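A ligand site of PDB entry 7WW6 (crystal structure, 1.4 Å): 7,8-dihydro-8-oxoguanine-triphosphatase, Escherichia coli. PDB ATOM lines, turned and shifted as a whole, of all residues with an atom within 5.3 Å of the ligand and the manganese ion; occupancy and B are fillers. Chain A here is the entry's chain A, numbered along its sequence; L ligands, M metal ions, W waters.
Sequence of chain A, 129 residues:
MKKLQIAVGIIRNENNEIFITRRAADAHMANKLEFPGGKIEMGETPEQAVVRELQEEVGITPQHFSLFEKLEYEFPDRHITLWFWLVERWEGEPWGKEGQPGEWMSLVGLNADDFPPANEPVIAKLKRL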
ATOM      1  N   ILE A   6      30.134 -20.523 -20.631  1.00  0.00           N
ATOM      2  CA  ILE A   6      30.420 -20.147 -22.024  1.00  0.00           C
ATOM      3  C   ILE A   6      29.698 -18.842 -22.330  1.00  0.00           C
ATOM      4  O   ILE A   6      28.502 -18.722 -22.064  1.00  0.00           O
ATOM      5  CB  ILE A   6      29.941 -21.245 -22.989  1.00  0.00           C
ATOM      6  CG1 ILE A   6      30.528 -22.621 -22.655  1.00  0.00           C
ATOM      7  CG2 ILE A   6      30.235 -20.841 -24.431  1.00  0.00           C
ATOM      8  CD1 ILE A   6      32.038 -22.703 -22.698  1.00  0.00           C
ATOM      9  N   VAL A   8      28.676 -16.326 -25.496  1.00  0.00           N
ATOM     10  CA  VAL A   8      28.573 -16.272 -26.945  1.00  0.00           C
ATOM     11  C   VAL A   8      27.874 -14.997 -27.380  1.00  0.00           C
ATOM     12  O   VAL A   8      27.107 -14.387 -26.624  1.00  0.00           O
ATOM     13  CB  VAL A   8      27.866 -17.507 -27.556  1.00  0.00           C
ATOM     14  CG1 VAL A   8      28.427 -18.798 -26.971  1.00  0.00           C
ATOM     15  CG2 VAL A   8      26.365 -17.438 -27.336  1.00  0.00           C
ATOM     16  N   ARG A  23      31.591 -25.055 -36.421  1.00  0.00           N
ATOM     17  CA  ARG A  23      32.599 -25.647 -35.559  1.00  0.00           C
ATOM     18  C   ARG A  23      33.402 -26.716 -36.295  1.00  0.00           C
ATOM     19  O   ARG A  23      32.885 -27.423 -37.167  1.00  0.00           O
ATOM     20  CB  ARG A  23      31.941 -26.232 -34.312  1.00  0.00           C
ATOM     21  CG  ARG A  23      31.236 -25.172 -33.489  1.00  0.00           C
ATOM     22  CD  ARG A  23      30.583 -25.713 -32.230  1.00  0.00           C
ATOM     23  NE  ARG A  23      31.523 -26.341 -31.313  1.00  0.00           N
ATOM     24  CZ  ARG A  23      32.295 -25.688 -30.448  1.00  0.00           C
ATOM     25  NH1 ARG A  23      32.286 -24.361 -30.400  1.00  0.00           N
ATOM     26  NH2 ARG A  23      33.098 -26.372 -29.648  1.00  0.00           N
ATOM     27  N   HIS A  28      34.131 -30.476 -29.768  1.00  0.00           N
ATOM     28  CA  HIS A  28      32.835 -30.774 -29.176  1.00  0.00           C
ATOM     29  C   HIS A  28      31.777 -30.067 -30.000  1.00  0.00           C
ATOM     30  O   HIS A  28      31.986 -28.949 -30.473  1.00  0.00           O
ATOM     31  CB  HIS A  28      32.768 -30.303 -27.729  1.00  0.00           C
ATOM     32  CG  HIS A  28      31.493 -30.694 -27.039  1.00  0.00           C
ATOM     33  ND1 HIS A  28      30.520 -29.783 -26.697  1.00  0.00           N
ATOM     34  CD2 HIS A  28      31.024 -31.908 -26.672  1.00  0.00           C
ATOM     35  CE1 HIS A  28      29.512 -30.423 -26.135  1.00  0.00           C
ATOM     36  NE2 HIS A  28      29.784 -31.711 -26.107  1.00  0.00           N
ATOM     37  N   MET A  29      30.632 -30.725 -30.205  1.00  0.00           N
ATOM     38  CA  MET A  29      29.612 -30.224 -31.132  1.00  0.00           C
ATOM     39  C   MET A  29      30.207 -29.999 -32.529  1.00  0.00           C
ATOM     40  O   MET A  29      30.017 -28.959 -33.155  1.00  0.00           O
ATOM     41  CB  MET A  29      28.898 -28.984 -30.601  1.00  0.00           C
ATOM     42  CG  MET A  29      27.959 -29.287 -29.424  1.00  0.00           C
ATOM     43  SD  MET A  29      26.575 -30.326 -29.948  1.00  0.00           S
ATOM     44  CE  MET A  29      26.982 -31.923 -29.246  1.00  0.00           C
ATOM     45  N   LEU A  33      26.670 -25.407 -36.598  1.00  0.00           N
ATOM     46  CA  LEU A  33      26.626 -23.960 -36.610  1.00  0.00           C
ATOM     47  C   LEU A  33      26.594 -23.448 -35.184  1.00  0.00           C
ATOM     48  O   LEU A  33      26.163 -24.146 -34.261  1.00  0.00           O
ATOM     49  CB  LEU A  33      25.401 -23.456 -37.372  1.00  0.00           C
ATOM     50  CG  LEU A  33      25.392 -23.791 -38.869  1.00  0.00           C
ATOM     51  CD1 LEU A  33      24.168 -23.183 -39.528  1.00  0.00           C
ATOM     52  CD2 LEU A  33      26.674 -23.342 -39.568  1.00  0.00           C
ATOM     53  N   GLU A  34      27.053 -22.213 -34.997  1.00  0.00           N
ATOM     54  CA  GLU A  34      27.231 -21.699 -33.643  1.00  0.00           C
ATOM     55  C   GLU A  34      27.258 -20.176 -33.668  1.00  0.00           C
ATOM     56  O   GLU A  34      27.622 -19.564 -34.680  1.00  0.00           O
ATOM     57  CB  GLU A  34      28.553 -22.194 -33.042  1.00  0.00           C
ATOM     58  CG  GLU A  34      29.735 -21.817 -33.910  1.00  0.00           C
ATOM     59  CD  GLU A  34      31.078 -21.897 -33.232  1.00  0.00           C
ATOM     60  OE1 GLU A  34      31.134 -22.291 -32.042  1.00  0.00           O
ATOM     61  OE2 GLU A  34      32.078 -21.563 -33.908  1.00  0.00           O
ATOM     62  N   PHE A  35      26.885 -19.574 -32.535  1.00  0.00           N
ATOM     63  CA  PHE A  35      27.238 -18.188 -32.292  1.00  0.00           C
ATOM     64  C   PHE A  35      28.695 -18.137 -31.833  1.00  0.00           C
ATOM     65  O   PHE A  35      29.088 -18.927 -30.980  1.00  0.00           O
ATOM     66  CB  PHE A  35      26.339 -17.593 -31.209  1.00  0.00           C
ATOM     67  CG  PHE A  35      24.869 -17.754 -31.486  1.00  0.00           C
ATOM     68  CD1 PHE A  35      24.286 -17.177 -32.613  1.00  0.00           C
ATOM     69  CD2 PHE A  35      24.067 -18.478 -30.626  1.00  0.00           C
ATOM     70  CE1 PHE A  35      22.924 -17.319 -32.863  1.00  0.00           C
ATOM     71  CE2 PHE A  35      22.711 -18.626 -30.864  1.00  0.00           C
ATOM     72  CZ  PHE A  35      22.137 -18.069 -31.988  1.00  0.00           C
ATOM     73  N   PRO A  36      29.522 -17.230 -32.357  1.00  0.00           N
ATOM     74  CA  PRO A  36      30.915 -17.173 -31.882  1.00  0.00           C
ATOM     75  C   PRO A  36      30.964 -16.953 -30.375  1.00  0.00           C
ATOM     76  O   PRO A  36      30.137 -16.246 -29.800  1.00  0.00           O
ATOM     77  CB  PRO A  36      31.497 -15.979 -32.654  1.00  0.00           C
ATOM     78  CG  PRO A  36      30.654 -15.900 -33.908  1.00  0.00           C
ATOM     79  CD  PRO A  36      29.256 -16.233 -33.414  1.00  0.00           C
ATOM     80  N   GLY A  37      31.930 -17.603 -29.719  1.00  0.00           N
ATOM     81  CA  GLY A  37      32.066 -17.444 -28.283  1.00  0.00           C
ATOM     82  C   GLY A  37      32.995 -18.497 -27.708  1.00  0.00           C
ATOM     83  O   GLY A  37      33.646 -19.240 -28.441  1.00  0.00           O
ATOM     84  N   GLY A  38      33.044 -18.564 -26.386  1.00  0.00           N
ATOM     85  CA  GLY A  38      33.894 -19.549 -25.749  1.00  0.00           C
ATOM     86  C   GLY A  38      33.899 -19.422 -24.242  1.00  0.00           C
ATOM     87  O   GLY A  38      33.066 -18.750 -23.648  1.00  0.00           O
ATOM     88  N   LYS A  39      34.888 -20.078 -23.642  1.00  0.00           N
ATOM     89  CA  LYS A  39      34.933 -20.262 -22.198  1.00  0.00           C
ATOM     90  C   LYS A  39      35.233 -18.951 -21.462  1.00  0.00           C
ATOM     91  O   LYS A  39      36.187 -18.239 -21.800  1.00  0.00           O
ATOM     92  CB  LYS A  39      35.993 -21.304 -21.858  1.00  0.00           C
ATOM     93  CG  LYS A  39      35.626 -22.687 -22.341  1.00  0.00           C
ATOM     94  CD  LYS A  39      36.828 -23.599 -22.534  1.00  0.00           C
ATOM     95  CE  LYS A  39      36.383 -24.934 -23.119  1.00  0.00           C
ATOM     96  NZ  LYS A  39      37.479 -25.708 -23.750  1.00  0.00           N
ATOM     97  N   GLU A  53      36.167 -13.048 -26.592  1.00  0.00           N
ATOM     98  CA  GLU A  53      35.914 -14.165 -27.501  1.00  0.00           C
ATOM     99  C   GLU A  53      35.578 -13.674 -28.906  1.00  0.00           C
ATOM    100  O   GLU A  53      36.054 -14.262 -29.899  1.00  0.00           O
ATOM    101  CB  GLU A  53      34.805 -15.043 -26.934  1.00  0.00           C
ATOM    102  CG  GLU A  53      35.233 -15.924 -25.774  1.00  0.00           C
ATOM    103  CD  GLU A  53      36.185 -17.028 -26.194  1.00  0.00           C
ATOM    104  OE1 GLU A  53      36.247 -17.340 -27.405  1.00  0.00           O
ATOM    105  OE2 GLU A  53      36.888 -17.582 -25.326  1.00  0.00           O
ATOM    106  N   GLU A  57      37.772 -14.670 -32.076  1.00  0.00           N
ATOM    107  CA  GLU A  57      37.224 -15.580 -33.069  1.00  0.00           C
ATOM    108  C   GLU A  57      36.835 -14.885 -34.374  1.00  0.00           C
ATOM    109  O   GLU A  57      37.026 -15.458 -35.449  1.00  0.00           O
ATOM    110  CB  GLU A  57      36.023 -16.344 -32.505  1.00  0.00           C
ATOM    111  CG  GLU A  57      36.439 -17.323 -31.441  1.00  0.00           C
ATOM    112  CD  GLU A  57      35.426 -18.413 -31.169  1.00  0.00           C
ATOM    113  OE1 GLU A  57      34.273 -18.303 -31.655  1.00  0.00           O
ATOM    114  OE2 GLU A  57      35.783 -19.396 -30.481  1.00  0.00           O
ATOM    115  N   PHE A  75      25.056 -31.902 -21.698  1.00  0.00           N
ATOM    116  CA  PHE A  75      25.490 -32.738 -22.795  1.00  0.00           C
ATOM    117  C   PHE A  75      25.865 -34.103 -22.246  1.00  0.00           C
ATOM    118  O   PHE A  75      25.977 -34.294 -21.032  1.00  0.00           O
ATOM    119  CB  PHE A  75      26.712 -32.095 -23.447  1.00  0.00           C
ATOM    120  CG  PHE A  75      26.398 -30.905 -24.300  1.00  0.00           C
ATOM    121  CD1 PHE A  75      25.915 -31.071 -25.586  1.00  0.00           C
ATOM    122  CD2 PHE A  75      26.614 -29.625 -23.823  1.00  0.00           C
ATOM    123  CE1 PHE A  75      25.634 -29.973 -26.390  1.00  0.00           C
ATOM    124  CE2 PHE A  75      26.339 -28.519 -24.625  1.00  0.00           C
ATOM    125  CZ  PHE A  75      25.850 -28.693 -25.913  1.00  0.00           C
ATOM    126  N   ARG A  78      29.373 -33.360 -20.446  1.00  0.00           N
ATOM    127  CA  ARG A  78      29.739 -32.086 -19.828  1.00  0.00           C
ATOM    128  C   ARG A  78      28.490 -31.273 -19.586  1.00  0.00           C
ATOM    129  O   ARG A  78      27.487 -31.412 -20.293  1.00  0.00           O
ATOM    130  CB  ARG A  78      30.736 -31.301 -20.681  1.00  0.00           C
ATOM    131  CG  ARG A  78      30.196 -30.863 -22.034  1.00  0.00           C
ATOM    132  CD  ARG A  78      31.333 -30.504 -22.975  1.00  0.00           C
ATOM    133  NE  ARG A  78      32.095 -31.694 -23.350  1.00  0.00           N
ATOM    134  CZ  ARG A  78      33.280 -31.672 -23.959  1.00  0.00           C
ATOM    135  NH1 ARG A  78      33.864 -30.515 -24.246  1.00  0.00           N
ATOM    136  NH2 ARG A  78      33.889 -32.806 -24.259  1.00  0.00           N
ATOM    137  N   ILE A  80      27.161 -27.377 -19.355  1.00  0.00           N
ATOM    138  CA  ILE A  80      27.559 -26.014 -19.658  1.00  0.00           C
ATOM    139  C   ILE A  80      26.455 -25.057 -19.266  1.00  0.00           C
ATOM    140  O   ILE A  80      25.265 -25.410 -19.205  1.00  0.00           O
ATOM    141  CB  ILE A  80      28.026 -25.790 -21.108  1.00  0.00           C
ATOM    142  CG1 ILE A  80      26.858 -25.881 -22.072  1.00  0.00           C
ATOM    143  CG2 ILE A  80      29.124 -26.783 -21.481  1.00  0.00           C
ATOM    144  CD1 ILE A  80      27.232 -25.447 -23.443  1.00  0.00           C
ATOM    145  N   LEU A  82      25.364 -21.378 -20.718  1.00  0.00           N
ATOM    146  CA  LEU A  82      25.568 -20.518 -21.874  1.00  0.00           C
ATOM    147  C   LEU A  82      24.982 -19.146 -21.620  1.00  0.00           C
ATOM    148  O   LEU A  82      23.818 -19.023 -21.222  1.00  0.00           O
ATOM    149  CB  LEU A  82      24.897 -21.127 -23.114  1.00  0.00           C
ATOM    150  CG  LEU A  82      25.672 -22.249 -23.785  1.00  0.00           C
ATOM    151  CD1 LEU A  82      24.702 -23.254 -24.390  1.00  0.00           C
ATOM    152  CD2 LEU A  82      26.601 -21.722 -24.871  1.00  0.00           C
ATOM    153  N   PHE A  84      24.044 -15.998 -23.672  1.00  0.00           N
ATOM    154  CA  PHE A  84      23.790 -15.557 -25.046  1.00  0.00           C
ATOM    155  C   PHE A  84      23.617 -14.050 -25.028  1.00  0.00           C
ATOM    156  O   PHE A  84      22.597 -13.549 -24.543  1.00  0.00           O
ATOM    157  CB  PHE A  84      22.520 -16.199 -25.613  1.00  0.00           C
ATOM    158  CG  PHE A  84      22.606 -17.691 -25.796  1.00  0.00           C
ATOM    159  CD1 PHE A  84      22.261 -18.543 -24.759  1.00  0.00           C
ATOM    160  CD2 PHE A  84      22.971 -18.234 -27.024  1.00  0.00           C
ATOM    161  CE1 PHE A  84      22.304 -19.919 -24.933  1.00  0.00           C
ATOM    162  CE2 PHE A  84      23.019 -19.603 -27.197  1.00  0.00           C
ATOM    163  CZ  PHE A  84      22.691 -20.444 -26.145  1.00  0.00           C
ATOM    164  N   PHE A 115      22.380 -26.336 -35.130  1.00  0.00           N
ATOM    165  CA  PHE A 115      23.102 -25.794 -33.990  1.00  0.00           C
ATOM    166  C   PHE A 115      23.135 -26.825 -32.867  1.00  0.00           C
ATOM    167  O   PHE A 115      22.370 -27.802 -32.894  1.00  0.00           O
ATOM    168  CB  PHE A 115      22.370 -24.536 -33.494  1.00  0.00           C
ATOM    169  CG  PHE A 115      22.486 -23.351 -34.404  1.00  0.00           C
ATOM    170  CD1 PHE A 115      21.705 -23.250 -35.539  1.00  0.00           C
ATOM    171  CD2 PHE A 115      23.392 -22.334 -34.114  1.00  0.00           C
ATOM    172  CE1 PHE A 115      21.814 -22.148 -36.368  1.00  0.00           C
ATOM    173  CE2 PHE A 115      23.499 -21.232 -34.933  1.00  0.00           C
ATOM    174  CZ  PHE A 115      22.713 -21.139 -36.070  1.00  0.00           C
ATOM    175  N   PRO A 116      23.979 -26.641 -31.850  1.00  0.00           N
ATOM    176  CA  PRO A 116      23.909 -27.522 -30.682  1.00  0.00           C
ATOM    177  C   PRO A 116      22.524 -27.454 -30.071  1.00  0.00           C
ATOM    178  O   PRO A 116      21.856 -26.402 -30.127  1.00  0.00           O
ATOM    179  CB  PRO A 116      24.967 -26.934 -29.735  1.00  0.00           C
ATOM    180  CG  PRO A 116      25.906 -26.189 -30.623  1.00  0.00           C
ATOM    181  CD  PRO A 116      25.030 -25.614 -31.700  1.00  0.00           C
ATOM    182  N   ALA A 118      21.472 -27.153 -27.181  1.00  0.00           N
ATOM    183  CA  ALA A 118      21.314 -26.127 -26.159  1.00  0.00           C
ATOM    184  C   ALA A 118      20.750 -24.836 -26.735  1.00  0.00           C
ATOM    185  O   ALA A 118      20.130 -24.052 -26.004  1.00  0.00           O
ATOM    186  CB  ALA A 118      22.668 -25.854 -25.499  1.00  0.00           C
ATOM    187  N   ASN A 119      20.969 -24.566 -28.020  1.00  0.00           N
ATOM    188  CA  ASN A 119      20.557 -23.302 -28.620  1.00  0.00           C
ATOM    189  C   ASN A 119      19.078 -23.254 -29.002  1.00  0.00           C
ATOM    190  O   ASN A 119      18.614 -22.176 -29.388  1.00  0.00           O
ATOM    191  CB  ASN A 119      21.381 -23.006 -29.866  1.00  0.00           C
ATOM    192  CG  ASN A 119      22.837 -22.717 -29.562  1.00  0.00           C
ATOM    193  OD1 ASN A 119      23.347 -23.116 -28.526  1.00  0.00           O
ATOM    194  ND2 ASN A 119      23.507 -22.002 -30.476  1.00  0.00           N
HETATM  195  P1  LIG L   1      39.138 -23.213 -26.541  1.00  0.00           P
HETATM  196  O1  LIG L   1      39.321 -24.243 -25.453  1.00  0.00           O
HETATM  197  O2  LIG L   1      39.421 -21.802 -26.099  1.00  0.00           O
HETATM  198  O3  LIG L   1      39.746 -23.614 -27.863  1.00  0.00           O
HETATM  199  O4  LIG L   1      37.551 -23.264 -26.837  1.00  0.00           O
HETATM  200  P2  LIG L   1      36.533 -22.017 -26.692  1.00  0.00           P
HETATM  201  O5  LIG L   1      36.843 -21.193 -25.459  1.00  0.00           O
HETATM  202  O6  LIG L   1      36.342 -21.298 -28.009  1.00  0.00           O
HETATM  203  O7  LIG L   1      35.218 -22.843 -26.311  1.00  0.00           O
HETATM  204  P3  LIG L   1      34.138 -23.508 -27.294  1.00  0.00           P
HETATM  205  O8  LIG L   1      33.505 -22.456 -28.196  1.00  0.00           O
HETATM  206  O9  LIG L   1      34.706 -24.739 -27.924  1.00  0.00           O
HETATM  207  O10 LIG L   1      33.121 -23.961 -26.148  1.00  0.00           O
HETATM  208  C1  LIG L   1      31.728 -23.792 -26.364  1.00  0.00           C
HETATM  209  C2  LIG L   1      30.966 -24.926 -25.710  1.00  0.00           C
HETATM  210  O11 LIG L   1      29.607 -24.533 -25.660  1.00  0.00           O
HETATM  211  C3  LIG L   1      31.014 -26.192 -26.543  1.00  0.00           C
HETATM  212  O12 LIG L   1      30.810 -27.300 -25.655  1.00  0.00           O
HETATM  213  C4  LIG L   1      29.815 -26.063 -27.443  1.00  0.00           C
HETATM  214  C5  LIG L   1      28.833 -25.317 -26.546  1.00  0.00           C
HETATM  215  N1  LIG L   1      27.940 -24.460 -27.338  1.00  0.00           N
HETATM  216  C6  LIG L   1      26.601 -24.587 -27.479  1.00  0.00           C
HETATM  217  N2  LIG L   1      26.043 -23.648 -28.249  1.00  0.00           N
HETATM  218  C7  LIG L   1      27.109 -22.833 -28.631  1.00  0.00           C
HETATM  219  C8  LIG L   1      27.203 -21.697 -29.453  1.00  0.00           C
HETATM  220  O13 LIG L   1      26.229 -21.175 -30.049  1.00  0.00           O
HETATM  221  N3  LIG L   1      28.462 -21.135 -29.580  1.00  0.00           N
HETATM  222  C9  LIG L   1      29.593 -21.668 -28.986  1.00  0.00           C
HETATM  223  N4  LIG L   1      30.788 -21.067 -29.149  1.00  0.00           N
HETATM  224  N5  LIG L   1      29.488 -22.772 -28.228  1.00  0.00           N
HETATM  225  C10 LIG L   1      28.278 -23.339 -28.058  1.00  0.00           C
HETATM  226  O14 LIG L   1      25.956 -25.514 -26.930  1.00  0.00           O
HETATM  227 MN    MN M   1      34.641 -20.932 -29.396  1.00  0.00          MN
HETATM  228  O   HOH W   1      36.709 -24.788 -29.771  1.00  0.00           O
HETATM  229  O   HOH W   2      37.767 -19.196 -28.105  1.00  0.00           O
HETATM  230  O   HOH W   3      35.015 -27.016 -26.257  1.00  0.00           O
HETATM  231  O   HOH W   4      35.501 -22.459 -30.839  1.00  0.00           O
HETATM  232  O   HOH W   5      33.188 -27.796 -24.314  1.00  0.00           O
HETATM  233  O   HOH W   6      41.268 -20.366 -27.862  1.00  0.00           O
HETATM  234  O   HOH W   7      33.004 -20.612 -30.922  1.00  0.00           O
HETATM  235  O   HOH W   8      38.237 -20.614 -30.801  1.00  0.00           O
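The side-chain amino group of Lys 39 lies within salt-bridge range of an oxygen (O1) of the ligand (2.9 Å).
N4 of the ligand lies within hydrogen-bond range of OE1 of Glu 34 (3.2 Å).
The backbone carbonyl oxygen (O) of Phe 35 is in hydrogen-bond range of a nitrogen (N3) of the ligand, at 2.7 Å.
OD1 of Asn 119 lies within hydrogen-bond range of N2 of the ligand (2.8 Å).
The backbone NH (N) of Lys 39 lies within hydrogen-bond range of an oxygen (O5) of the ligand (2.9 Å).
ND1 of His 28 is in hydrogen-bond range of O12 of the ligand (2.7 Å).
The backbone NH of Phe 35 sits at hydrogen-bond distance from an oxygen (O13) of the ligand (3.0 Å).
The guanidinium group (NH2) of Arg 23 lies within salt-bridge range of an oxygen (O9) of the ligand (2.9 Å).
The backbone carbonyl oxygen of His 28 lies within hydrogen-bond range of the guanidinium group of Arg 23.
The side-chain carboxylate (OE1) of Glu 34 is in salt-bridge range of the guanidinium group (NH1) of Arg 23 (2.9 Å).
Residues that only touch the ligand: Ile 6, Val 8, Gly 38, Glu 53, Phe 75, Ile 80, Leu 82, Pro 116 and Ala 118.
Within 4 Å of the ligand: Ile 6, Val 8, Arg 23, His 28, Glu 34, Phe 35, Gly 37, Gly 38, Lys 39, Glu 53, Glu 57, Phe 75, Ile 80, Leu 82, Pro 116, Ala 118 and Asn 119.
The nearest printed residue that does not touch the ligand is Arg 78 (4.2 Å).
Gly 38 touches the manganese ion (CA to MN, 3.97 Å).
Within 4 Å of the manganese ion: Gly 37, Gly 38 and Glu 57.
The nearest printed residue that does not touch the manganese ion is Arg 23 (4.3 Å).
The manganese ion is bound by O of Gly 37.
The manganese ion is bound by OE2 of Glu 57 (2.2 Å).
O6 of the ligand binds the manganese ion (2.2 Å).
An oxygen (O8) of the ligand is bound to the manganese ion (2.2 Å).
Water W7 binds the manganese ion, at 2.3 Å.
Water W4 is bound to the manganese ion (2.3 Å).
The manganese ion has six donor atoms within binding distance.
Water W7 lies within hydrogen-bond range of the side-chain carboxylate of Glu 57, the side-chain carboxylate of Glu 34, a nitrogen (N4) of the ligand and the backbone NH of Gly 37.
Water W2 bridges the side-chain carboxylate (OE1) of Glu 53 (2.5 Å) and an oxygen (O5) of the ligand (3.4 Å).
Water W5 bridges O12 of the ligand (2.8 Å) and NH1 of Arg 78 (2.8 Å).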
